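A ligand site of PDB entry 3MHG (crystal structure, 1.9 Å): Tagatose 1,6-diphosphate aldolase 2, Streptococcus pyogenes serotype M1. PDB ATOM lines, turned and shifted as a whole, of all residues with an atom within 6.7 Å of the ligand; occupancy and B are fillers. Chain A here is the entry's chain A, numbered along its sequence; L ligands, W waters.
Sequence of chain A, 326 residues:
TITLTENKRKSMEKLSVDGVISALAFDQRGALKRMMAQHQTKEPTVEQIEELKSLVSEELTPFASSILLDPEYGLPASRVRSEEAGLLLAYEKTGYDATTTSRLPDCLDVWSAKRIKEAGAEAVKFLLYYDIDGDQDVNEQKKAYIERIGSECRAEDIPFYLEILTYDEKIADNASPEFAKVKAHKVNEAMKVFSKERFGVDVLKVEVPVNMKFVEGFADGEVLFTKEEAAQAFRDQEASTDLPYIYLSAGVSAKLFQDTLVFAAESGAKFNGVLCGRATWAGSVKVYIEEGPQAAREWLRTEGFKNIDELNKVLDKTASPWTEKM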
ATOM      1  N   ALA A  25       5.130  -2.797  14.740  1.00  0.00           N
ATOM      2  CA  ALA A  25       6.128  -3.802  14.398  1.00  0.00           C
ATOM      3  C   ALA A  25       5.722  -4.573  13.158  1.00  0.00           C
ATOM      4  O   ALA A  25       4.639  -5.152  13.100  1.00  0.00           O
ATOM      5  CB  ALA A  25       6.338  -4.763  15.573  1.00  0.00           C
ATOM      6  N   PHE A  26       6.601  -4.594  12.153  1.00  0.00           N
ATOM      7  CA  PHE A  26       6.360  -5.397  10.961  1.00  0.00           C
ATOM      8  C   PHE A  26       7.650  -5.924  10.343  1.00  0.00           C
ATOM      9  O   PHE A  26       7.922  -5.719   9.155  1.00  0.00           O
ATOM     10  CB  PHE A  26       5.577  -4.596   9.909  1.00  0.00           C
ATOM     11  CG  PHE A  26       4.796  -5.457   8.954  1.00  0.00           C
ATOM     12  CD1 PHE A  26       4.714  -6.822   9.138  1.00  0.00           C
ATOM     13  CD2 PHE A  26       4.117  -4.882   7.882  1.00  0.00           C
ATOM     14  CE1 PHE A  26       3.992  -7.623   8.262  1.00  0.00           C
ATOM     15  CE2 PHE A  26       3.384  -5.675   7.007  1.00  0.00           C
ATOM     16  CZ  PHE A  26       3.319  -7.042   7.194  1.00  0.00           C
ATOM     17  N   ASP A  27       8.454  -6.595  11.157  1.00  0.00           N
ATOM     18  CA  ASP A  27       9.694  -7.191  10.646  1.00  0.00           C
ATOM     19  C   ASP A  27       9.514  -8.685  10.405  1.00  0.00           C
ATOM     20  O   ASP A  27      10.462  -9.391  10.079  1.00  0.00           O
ATOM     21  CB  ASP A  27      10.870  -6.928  11.581  1.00  0.00           C
ATOM     22  CG  ASP A  27      10.643  -7.458  12.985  1.00  0.00           C
ATOM     23  OD1 ASP A  27       9.502  -7.831  13.334  1.00  0.00           O
ATOM     24  OD2 ASP A  27      11.616  -7.477  13.767  1.00  0.00           O
ATOM     25  N   GLN A  28       8.280  -9.149  10.559  1.00  0.00           N
ATOM     26  CA  GLN A  28       7.961 -10.548  10.343  1.00  0.00           C
ATOM     27  C   GLN A  28       8.316 -10.955   8.916  1.00  0.00           C
ATOM     28  O   GLN A  28       8.005 -10.241   7.949  1.00  0.00           O
ATOM     29  CB  GLN A  28       6.485 -10.834  10.660  1.00  0.00           C
ATOM     30  CG  GLN A  28       6.146 -10.893  12.156  1.00  0.00           C
ATOM     31  CD  GLN A  28       5.947  -9.507  12.784  1.00  0.00           C
ATOM     32  OE1 GLN A  28       6.125  -8.479  12.129  1.00  0.00           O
ATOM     33  NE2 GLN A  28       5.567  -9.498  14.063  1.00  0.00           N
ATOM     34  N   LEU A  68       9.081  -0.647  13.184  1.00  0.00           N
ATOM     35  CA  LEU A  68      10.153  -1.632  13.104  1.00  0.00           C
ATOM     36  C   LEU A  68       9.973  -2.449  11.833  1.00  0.00           C
ATOM     37  O   LEU A  68       8.926  -3.056  11.613  1.00  0.00           O
ATOM     38  CB  LEU A  68      10.109  -2.548  14.326  1.00  0.00           C
ATOM     39  CG  LEU A  68      10.837  -3.889  14.210  1.00  0.00           C
ATOM     40  CD1 LEU A  68      12.328  -3.711  13.959  1.00  0.00           C
ATOM     41  CD2 LEU A  68      10.591  -4.702  15.478  1.00  0.00           C
ATOM     42  N   ALA A  90      15.414  -4.644  12.173  1.00  0.00           N
ATOM     43  CA  ALA A  90      15.771  -5.931  12.768  1.00  0.00           C
ATOM     44  C   ALA A  90      17.136  -6.422  12.292  1.00  0.00           C
ATOM     45  O   ALA A  90      17.536  -6.181  11.157  1.00  0.00           O
ATOM     46  CB  ALA A  90      14.703  -6.960  12.454  1.00  0.00           C
ATOM     47  N   GLU A  92      18.337  -9.743  13.472  1.00  0.00           N
ATOM     48  CA  GLU A  92      18.405 -11.195  13.581  1.00  0.00           C
ATOM     49  C   GLU A  92      17.817 -11.903  12.359  1.00  0.00           C
ATOM     50  O   GLU A  92      16.916 -11.384  11.708  1.00  0.00           O
ATOM     51  CB  GLU A  92      17.672 -11.676  14.843  1.00  0.00           C
ATOM     52  CG  GLU A  92      16.165 -11.848  14.667  1.00  0.00           C
ATOM     53  CD  GLU A  92      15.382 -10.545  14.778  1.00  0.00           C
ATOM     54  OE1 GLU A  92      15.976  -9.512  15.166  1.00  0.00           O
ATOM     55  OE2 GLU A  92      14.164 -10.550  14.489  1.00  0.00           O
ATOM     56  N   LYS A 125      17.298  -3.508  16.345  1.00  0.00           N
ATOM     57  CA  LYS A 125      16.462  -4.425  17.094  1.00  0.00           C
ATOM     58  C   LYS A 125      16.979  -5.849  16.877  1.00  0.00           C
ATOM     59  O   LYS A 125      17.346  -6.217  15.761  1.00  0.00           O
ATOM     60  CB  LYS A 125      14.997  -4.306  16.668  1.00  0.00           C
ATOM     61  CG  LYS A 125      14.071  -5.351  17.278  1.00  0.00           C
ATOM     62  CD  LYS A 125      13.911  -6.555  16.356  1.00  0.00           C
ATOM     63  CE  LYS A 125      13.069  -7.647  17.004  1.00  0.00           C
ATOM     64  NZ  LYS A 125      12.628  -8.661  15.998  1.00  0.00           N
ATOM     65  N   LEU A 127      16.170 -10.039  18.188  1.00  0.00           N
ATOM     66  CA  LEU A 127      15.341 -10.981  18.920  1.00  0.00           C
ATOM     67  C   LEU A 127      16.163 -12.163  19.438  1.00  0.00           C
ATOM     68  O   LEU A 127      16.883 -12.801  18.672  1.00  0.00           O
ATOM     69  CB  LEU A 127      14.194 -11.484  18.037  1.00  0.00           C
ATOM     70  CG  LEU A 127      13.471 -12.751  18.495  1.00  0.00           C
ATOM     71  CD1 LEU A 127      12.897 -12.590  19.891  1.00  0.00           C
ATOM     72  CD2 LEU A 127      12.370 -13.106  17.497  1.00  0.00           C
ATOM     73  N   GLU A 163      14.679  -7.735  21.975  1.00  0.00           N
ATOM     74  CA  GLU A 163      13.446  -8.469  22.201  1.00  0.00           C
ATOM     75  C   GLU A 163      13.794  -9.827  22.785  1.00  0.00           C
ATOM     76  O   GLU A 163      14.697 -10.524  22.296  1.00  0.00           O
ATOM     77  CB  GLU A 163      12.667  -8.661  20.891  1.00  0.00           C
ATOM     78  CG  GLU A 163      11.331  -9.375  21.078  1.00  0.00           C
ATOM     79  CD  GLU A 163      10.634  -9.690  19.750  1.00  0.00           C
ATOM     80  OE1 GLU A 163      11.128  -9.272  18.689  1.00  0.00           O
ATOM     81  OE2 GLU A 163       9.590 -10.371  19.782  1.00  0.00           O
ATOM     82  N   LEU A 165      12.020 -13.446  23.674  1.00  0.00           N
ATOM     83  CA  LEU A 165      10.902 -14.383  23.712  1.00  0.00           C
ATOM     84  C   LEU A 165      11.336 -15.591  24.516  1.00  0.00           C
ATOM     85  O   LEU A 165      12.348 -16.213  24.225  1.00  0.00           O
ATOM     86  CB  LEU A 165      10.497 -14.808  22.300  1.00  0.00           C
ATOM     87  CG  LEU A 165       9.799 -13.728  21.467  1.00  0.00           C
ATOM     88  CD1 LEU A 165       9.448 -14.275  20.093  1.00  0.00           C
ATOM     89  CD2 LEU A 165       8.546 -13.222  22.188  1.00  0.00           C
ATOM     90  N   LYS A 205      12.205  -5.189  24.704  1.00  0.00           N
ATOM     91  CA  LYS A 205      10.896  -5.513  24.153  1.00  0.00           C
ATOM     92  C   LYS A 205      10.521  -6.900  24.678  1.00  0.00           C
ATOM     93  O   LYS A 205      11.184  -7.871  24.345  1.00  0.00           O
ATOM     94  CB  LYS A 205      10.939  -5.529  22.628  1.00  0.00           C
ATOM     95  CG  LYS A 205       9.661  -6.024  21.970  1.00  0.00           C
ATOM     96  CD  LYS A 205       9.814  -6.071  20.449  1.00  0.00           C
ATOM     97  CE  LYS A 205       8.630  -6.775  19.801  1.00  0.00           C
ATOM     98  NZ  LYS A 205       8.777  -6.860  18.324  1.00  0.00           N
ATOM     99  N   TYR A 247       5.945  -3.645  25.556  1.00  0.00           N
ATOM    100  CA  TYR A 247       5.325  -4.950  25.343  1.00  0.00           C
ATOM    101  C   TYR A 247       5.111  -5.286  23.864  1.00  0.00           C
ATOM    102  O   TYR A 247       4.737  -4.441  23.066  1.00  0.00           O
ATOM    103  CB  TYR A 247       3.990  -5.036  26.071  1.00  0.00           C
ATOM    104  CG  TYR A 247       4.091  -5.036  27.575  1.00  0.00           C
ATOM    105  CD1 TYR A 247       4.900  -5.945  28.240  1.00  0.00           C
ATOM    106  CD2 TYR A 247       3.337  -4.146  28.341  1.00  0.00           C
ATOM    107  CE1 TYR A 247       4.989  -5.958  29.618  1.00  0.00           C
ATOM    108  CE2 TYR A 247       3.408  -4.149  29.727  1.00  0.00           C
ATOM    109  CZ  TYR A 247       4.241  -5.056  30.358  1.00  0.00           C
ATOM    110  OH  TYR A 247       4.318  -5.074  31.739  1.00  0.00           O
ATOM    111  N   LEU A 248       5.337  -6.565  23.533  1.00  0.00           N
ATOM    112  CA  LEU A 248       4.953  -7.107  22.241  1.00  0.00           C
ATOM    113  C   LEU A 248       3.560  -7.700  22.373  1.00  0.00           C
ATOM    114  O   LEU A 248       3.169  -8.090  23.461  1.00  0.00           O
ATOM    115  CB  LEU A 248       5.950  -8.200  21.813  1.00  0.00           C
ATOM    116  CG  LEU A 248       6.178  -9.330  22.824  1.00  0.00           C
ATOM    117  CD1 LEU A 248       5.309 -10.543  22.508  1.00  0.00           C
ATOM    118  CD2 LEU A 248       7.656  -9.738  22.828  1.00  0.00           C
ATOM    119  N   SER A 249       2.795  -7.778  21.274  1.00  0.00           N
ATOM    120  CA  SER A 249       1.412  -8.265  21.336  1.00  0.00           C
ATOM    121  C   SER A 249       1.310  -9.782  21.355  1.00  0.00           C
ATOM    122  O   SER A 249       0.336 -10.345  21.887  1.00  0.00           O
ATOM    123  CB  SER A 249       0.560  -7.703  20.187  1.00  0.00           C
ATOM    124  OG  SER A 249       0.835  -8.374  18.966  1.00  0.00           O
ATOM    125  N   ALA A 250       2.293 -10.454  20.768  1.00  0.00           N
ATOM    126  CA  ALA A 250       2.299 -11.907  20.681  1.00  0.00           C
ATOM    127  C   ALA A 250       1.163 -12.433  19.799  1.00  0.00           C
ATOM    128  O   ALA A 250       0.835 -13.612  19.834  1.00  0.00           O
ATOM    129  CB  ALA A 250       2.246 -12.546  22.086  1.00  0.00           C
ATOM    130  N   GLY A 251       0.587 -11.548  18.988  1.00  0.00           N
ATOM    131  CA  GLY A 251      -0.486 -11.925  18.082  1.00  0.00           C
ATOM    132  C   GLY A 251      -1.832 -12.219  18.725  1.00  0.00           C
ATOM    133  O   GLY A 251      -2.695 -12.836  18.101  1.00  0.00           O
ATOM    134  N   PHE A 257      -5.133  -7.379  23.806  1.00  0.00           N
ATOM    135  CA  PHE A 257      -3.893  -6.659  24.056  1.00  0.00           C
ATOM    136  C   PHE A 257      -4.191  -5.359  24.789  1.00  0.00           C
ATOM    137  O   PHE A 257      -3.555  -5.024  25.773  1.00  0.00           O
ATOM    138  CB  PHE A 257      -3.140  -6.384  22.757  1.00  0.00           C
ATOM    139  CG  PHE A 257      -1.729  -5.880  22.952  1.00  0.00           C
ATOM    140  CD1 PHE A 257      -0.840  -6.543  23.782  1.00  0.00           C
ATOM    141  CD2 PHE A 257      -1.286  -4.752  22.276  1.00  0.00           C
ATOM    142  CE1 PHE A 257       0.454  -6.087  23.954  1.00  0.00           C
ATOM    143  CE2 PHE A 257       0.010  -4.290  22.435  1.00  0.00           C
ATOM    144  CZ  PHE A 257       0.885  -4.964  23.279  1.00  0.00           C
ATOM    145  N   LEU A 275       5.825  -2.357  21.156  1.00  0.00           N
ATOM    146  CA  LEU A 275       6.156  -2.608  19.760  1.00  0.00           C
ATOM    147  C   LEU A 275       5.106  -3.623  19.331  1.00  0.00           C
ATOM    148  O   LEU A 275       5.255  -4.822  19.545  1.00  0.00           O
ATOM    149  CB  LEU A 275       7.575  -3.136  19.596  1.00  0.00           C
ATOM    150  CG  LEU A 275       8.524  -2.163  18.866  1.00  0.00           C
ATOM    151  CD1 LEU A 275       9.999  -2.584  18.942  1.00  0.00           C
ATOM    152  CD2 LEU A 275       8.097  -2.012  17.399  1.00  0.00           C
ATOM    153  N   CYS A 276       4.005  -3.115  18.795  1.00  0.00           N
ATOM    154  CA  CYS A 276       2.838  -3.937  18.525  1.00  0.00           C
ATOM    155  C   CYS A 276       2.726  -4.254  17.046  1.00  0.00           C
ATOM    156  O   CYS A 276       2.675  -3.359  16.210  1.00  0.00           O
ATOM    157  CB  CYS A 276       1.571  -3.219  19.011  1.00  0.00           C
ATOM    158  SG  CYS A 276       0.047  -4.152  18.714  1.00  0.00           S
ATOM    159  N   GLY A 277       2.697  -5.544  16.715  1.00  0.00           N
ATOM    160  CA  GLY A 277       2.657  -5.979  15.335  1.00  0.00           C
ATOM    161  C   GLY A 277       1.354  -6.636  14.948  1.00  0.00           C
ATOM    162  O   GLY A 277       0.409  -5.967  14.526  1.00  0.00           O
ATOM    163  N   ARG A 278       1.290  -7.950  15.095  1.00  0.00           N
ATOM    164  CA  ARG A 278       0.131  -8.727  14.650  1.00  0.00           C
ATOM    165  C   ARG A 278      -1.229  -8.260  15.179  1.00  0.00           C
ATOM    166  O   ARG A 278      -2.201  -8.244  14.427  1.00  0.00           O
ATOM    167  CB  ARG A 278       0.354 -10.218  14.943  1.00  0.00           C
ATOM    168  CG  ARG A 278       1.411 -10.847  14.030  1.00  0.00           C
ATOM    169  CD  ARG A 278       1.931 -12.163  14.625  1.00  0.00           C
ATOM    170  NE  ARG A 278       2.701 -11.938  15.844  1.00  0.00           N
ATOM    171  CZ  ARG A 278       3.071 -12.900  16.677  1.00  0.00           C
ATOM    172  NH1 ARG A 278       2.739 -14.158  16.433  1.00  0.00           N
ATOM    173  NH2 ARG A 278       3.773 -12.596  17.766  1.00  0.00           N
ATOM    174  N   ALA A 279      -1.306  -7.875  16.447  1.00  0.00           N
ATOM    175  CA  ALA A 279      -2.578  -7.412  17.011  1.00  0.00           C
ATOM    176  C   ALA A 279      -3.155  -6.265  16.188  1.00  0.00           C
ATOM    177  O   ALA A 279      -4.366  -6.064  16.155  1.00  0.00           O
ATOM    178  CB  ALA A 279      -2.419  -6.994  18.473  1.00  0.00           C
ATOM    179  N   THR A 280      -2.294  -5.504  15.526  1.00  0.00           N
ATOM    180  CA  THR A 280      -2.752  -4.366  14.726  1.00  0.00           C
ATOM    181  C   THR A 280      -3.061  -4.725  13.270  1.00  0.00           C
ATOM    182  O   THR A 280      -4.136  -4.402  12.770  1.00  0.00           O
ATOM    183  CB  THR A 280      -1.730  -3.220  14.749  1.00  0.00           C
ATOM    184  OG1 THR A 280      -1.622  -2.710  16.082  1.00  0.00           O
ATOM    185  CG2 THR A 280      -2.155  -2.078  13.808  1.00  0.00           C
ATOM    186  N   TRP A 281      -2.131  -5.414  12.616  1.00  0.00           N
ATOM    187  CA  TRP A 281      -2.208  -5.604  11.161  1.00  0.00           C
ATOM    188  C   TRP A 281      -2.579  -7.014  10.661  1.00  0.00           C
ATOM    189  O   TRP A 281      -2.712  -7.214   9.456  1.00  0.00           O
ATOM    190  CB  TRP A 281      -0.911  -5.132  10.474  1.00  0.00           C
ATOM    191  CG  TRP A 281       0.351  -5.828  10.925  1.00  0.00           C
ATOM    192  CD1 TRP A 281       1.370  -5.278  11.666  1.00  0.00           C
ATOM    193  CD2 TRP A 281       0.761  -7.176  10.654  1.00  0.00           C
ATOM    194  NE1 TRP A 281       2.362  -6.203  11.869  1.00  0.00           N
ATOM    195  CE2 TRP A 281       2.007  -7.376  11.263  1.00  0.00           C
ATOM    196  CE3 TRP A 281       0.163  -8.236   9.947  1.00  0.00           C
ATOM    197  CZ2 TRP A 281       2.689  -8.593  11.189  1.00  0.00           C
ATOM    198  CZ3 TRP A 281       0.851  -9.446   9.878  1.00  0.00           C
ATOM    199  CH2 TRP A 281       2.091  -9.608  10.501  1.00  0.00           C
HETATM  200  P1  LIG L   1       4.109  -8.793  17.691  1.00  0.00           P
HETATM  201  O1  LIG L   1       3.320  -9.404  16.386  1.00  0.00           O
HETATM  202  O2  LIG L   1       4.383  -9.991  18.777  1.00  0.00           O
HETATM  203  O3  LIG L   1       3.323  -7.727  18.328  1.00  0.00           O
HETATM  204  O4  LIG L   1       5.533  -8.158  17.175  1.00  0.00           O
HETATM  205  C1  LIG L   1       6.362  -7.541  18.097  1.00  0.00           C
HETATM  206  C2  LIG L   1       7.821  -7.469  17.691  1.00  0.00           C
HETATM  207  C3  LIG L   1       8.150  -8.012  16.309  1.00  0.00           C
HETATM  208  O5  LIG L   1       9.507  -8.128  15.995  1.00  0.00           O
HETATM  209  O   HOH W   1       6.706 -11.309  18.989  1.00  0.00           O
HETATM  210  O   HOH W   2       9.010 -11.272  16.815  1.00  0.00           O
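The backbone NH (N) of Ser 249 lies within hydrogen-bond range of an oxygen (O3) of the ligand, 3.0 Å away.
O1 of the ligand is in salt-bridge range of NE of Arg 278, at 2.7 Å.
An oxygen (O5) of the ligand sits at hydrogen-bond distance from the side-chain carboxylate (OD1) of Asp 27 (2.7 Å).
OG of Ser 249 is in hydrogen-bond range of O3 of the ligand (2.6 Å).
The side-chain carboxylate (OE1) of Glu 163 sits at hydrogen-bond distance from an oxygen (O5) of the ligand, at 3.3 Å.
The side-chain amino group (NZ) of Lys 205 is bonded to a carbon (C2) of the ligand (1.3 Å).
An oxygen (O1) of the ligand is in hydrogen-bond range of the backbone NH (N) of Arg 278 (2.8 Å).
The side-chain amide nitrogen (NE2) of Gln 28 lies within hydrogen-bond range of an oxygen (O1) of the ligand (3.2 Å).
An oxygen (O2) of the ligand sits at hydrogen-bond distance from the backbone NH of Ala 250, at 2.9 Å.
The side-chain amino group (NZ) of Lys 125 lies within hydrogen-bond range of an oxygen (O5) of the ligand, at 3.2 Å.
N of Gly 277 is in hydrogen-bond range of O3 of the ligand (2.8 Å).
The backbone carbonyl oxygen (O) of Ala 25 lies within hydrogen-bond range of the indole nitrogen (NE1) of Trp 281 (2.8 Å).
The backbone carbonyl oxygen (O) of Leu 68 lies within hydrogen-bond range of the backbone NH (N) of Phe 26, at 2.8 Å.
OE1 of Glu 163 lies within salt-bridge range of NZ of Lys 205.
The side-chain carboxylate of Glu 92 lies within salt-bridge range of the side-chain amino group of Lys 125 (2.9 Å).
OG of Ser 249 is in hydrogen-bond range of N of Ala 279 (3.3 Å).
The side-chain hydroxyl of Ser 249 sits close to the backbone NH of Gly 251 (3.2 Å).
SG of Cys 276 sits at hydrogen-bond distance from OG1 of Thr 280 (3.4 Å).
NZ of Lys 125 lies within salt-bridge range of OD2 of Asp 27 (2.7 Å).
Ala 25 touches the ligand.
Leu 68 touches the ligand (CD2 to O5, 3.6 Å).
CB of Leu 248 touches C1 of the ligand, at 3.8 Å.
Leu 275 touches the ligand.
C of Cys 276 touches O3 of the ligand, 3.7 Å away.
Hydrophobic or aromatic side chains within 4 Å of the ligand: Ala 25, Leu 68 and Leu 248.
14 residues have an atom within 4 Å of the ligand: Ala 25, Asp 27, Gln 28, Leu 68, Lys 125, Glu 163, Lys 205, Leu 248, Ser 249, Ala 250, Leu 275, Cys 276, Gly 277 and Arg 278.
The nearest printed residue that does not touch the ligand is Gly 251 (4.1 Å).
Water W1 lies within hydrogen-bond range of O2 of the ligand, OE2 of Glu 163 and NH2 of Arg 278.
Water W2 bridges OE2 of Glu 163 and O5 of the ligand.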
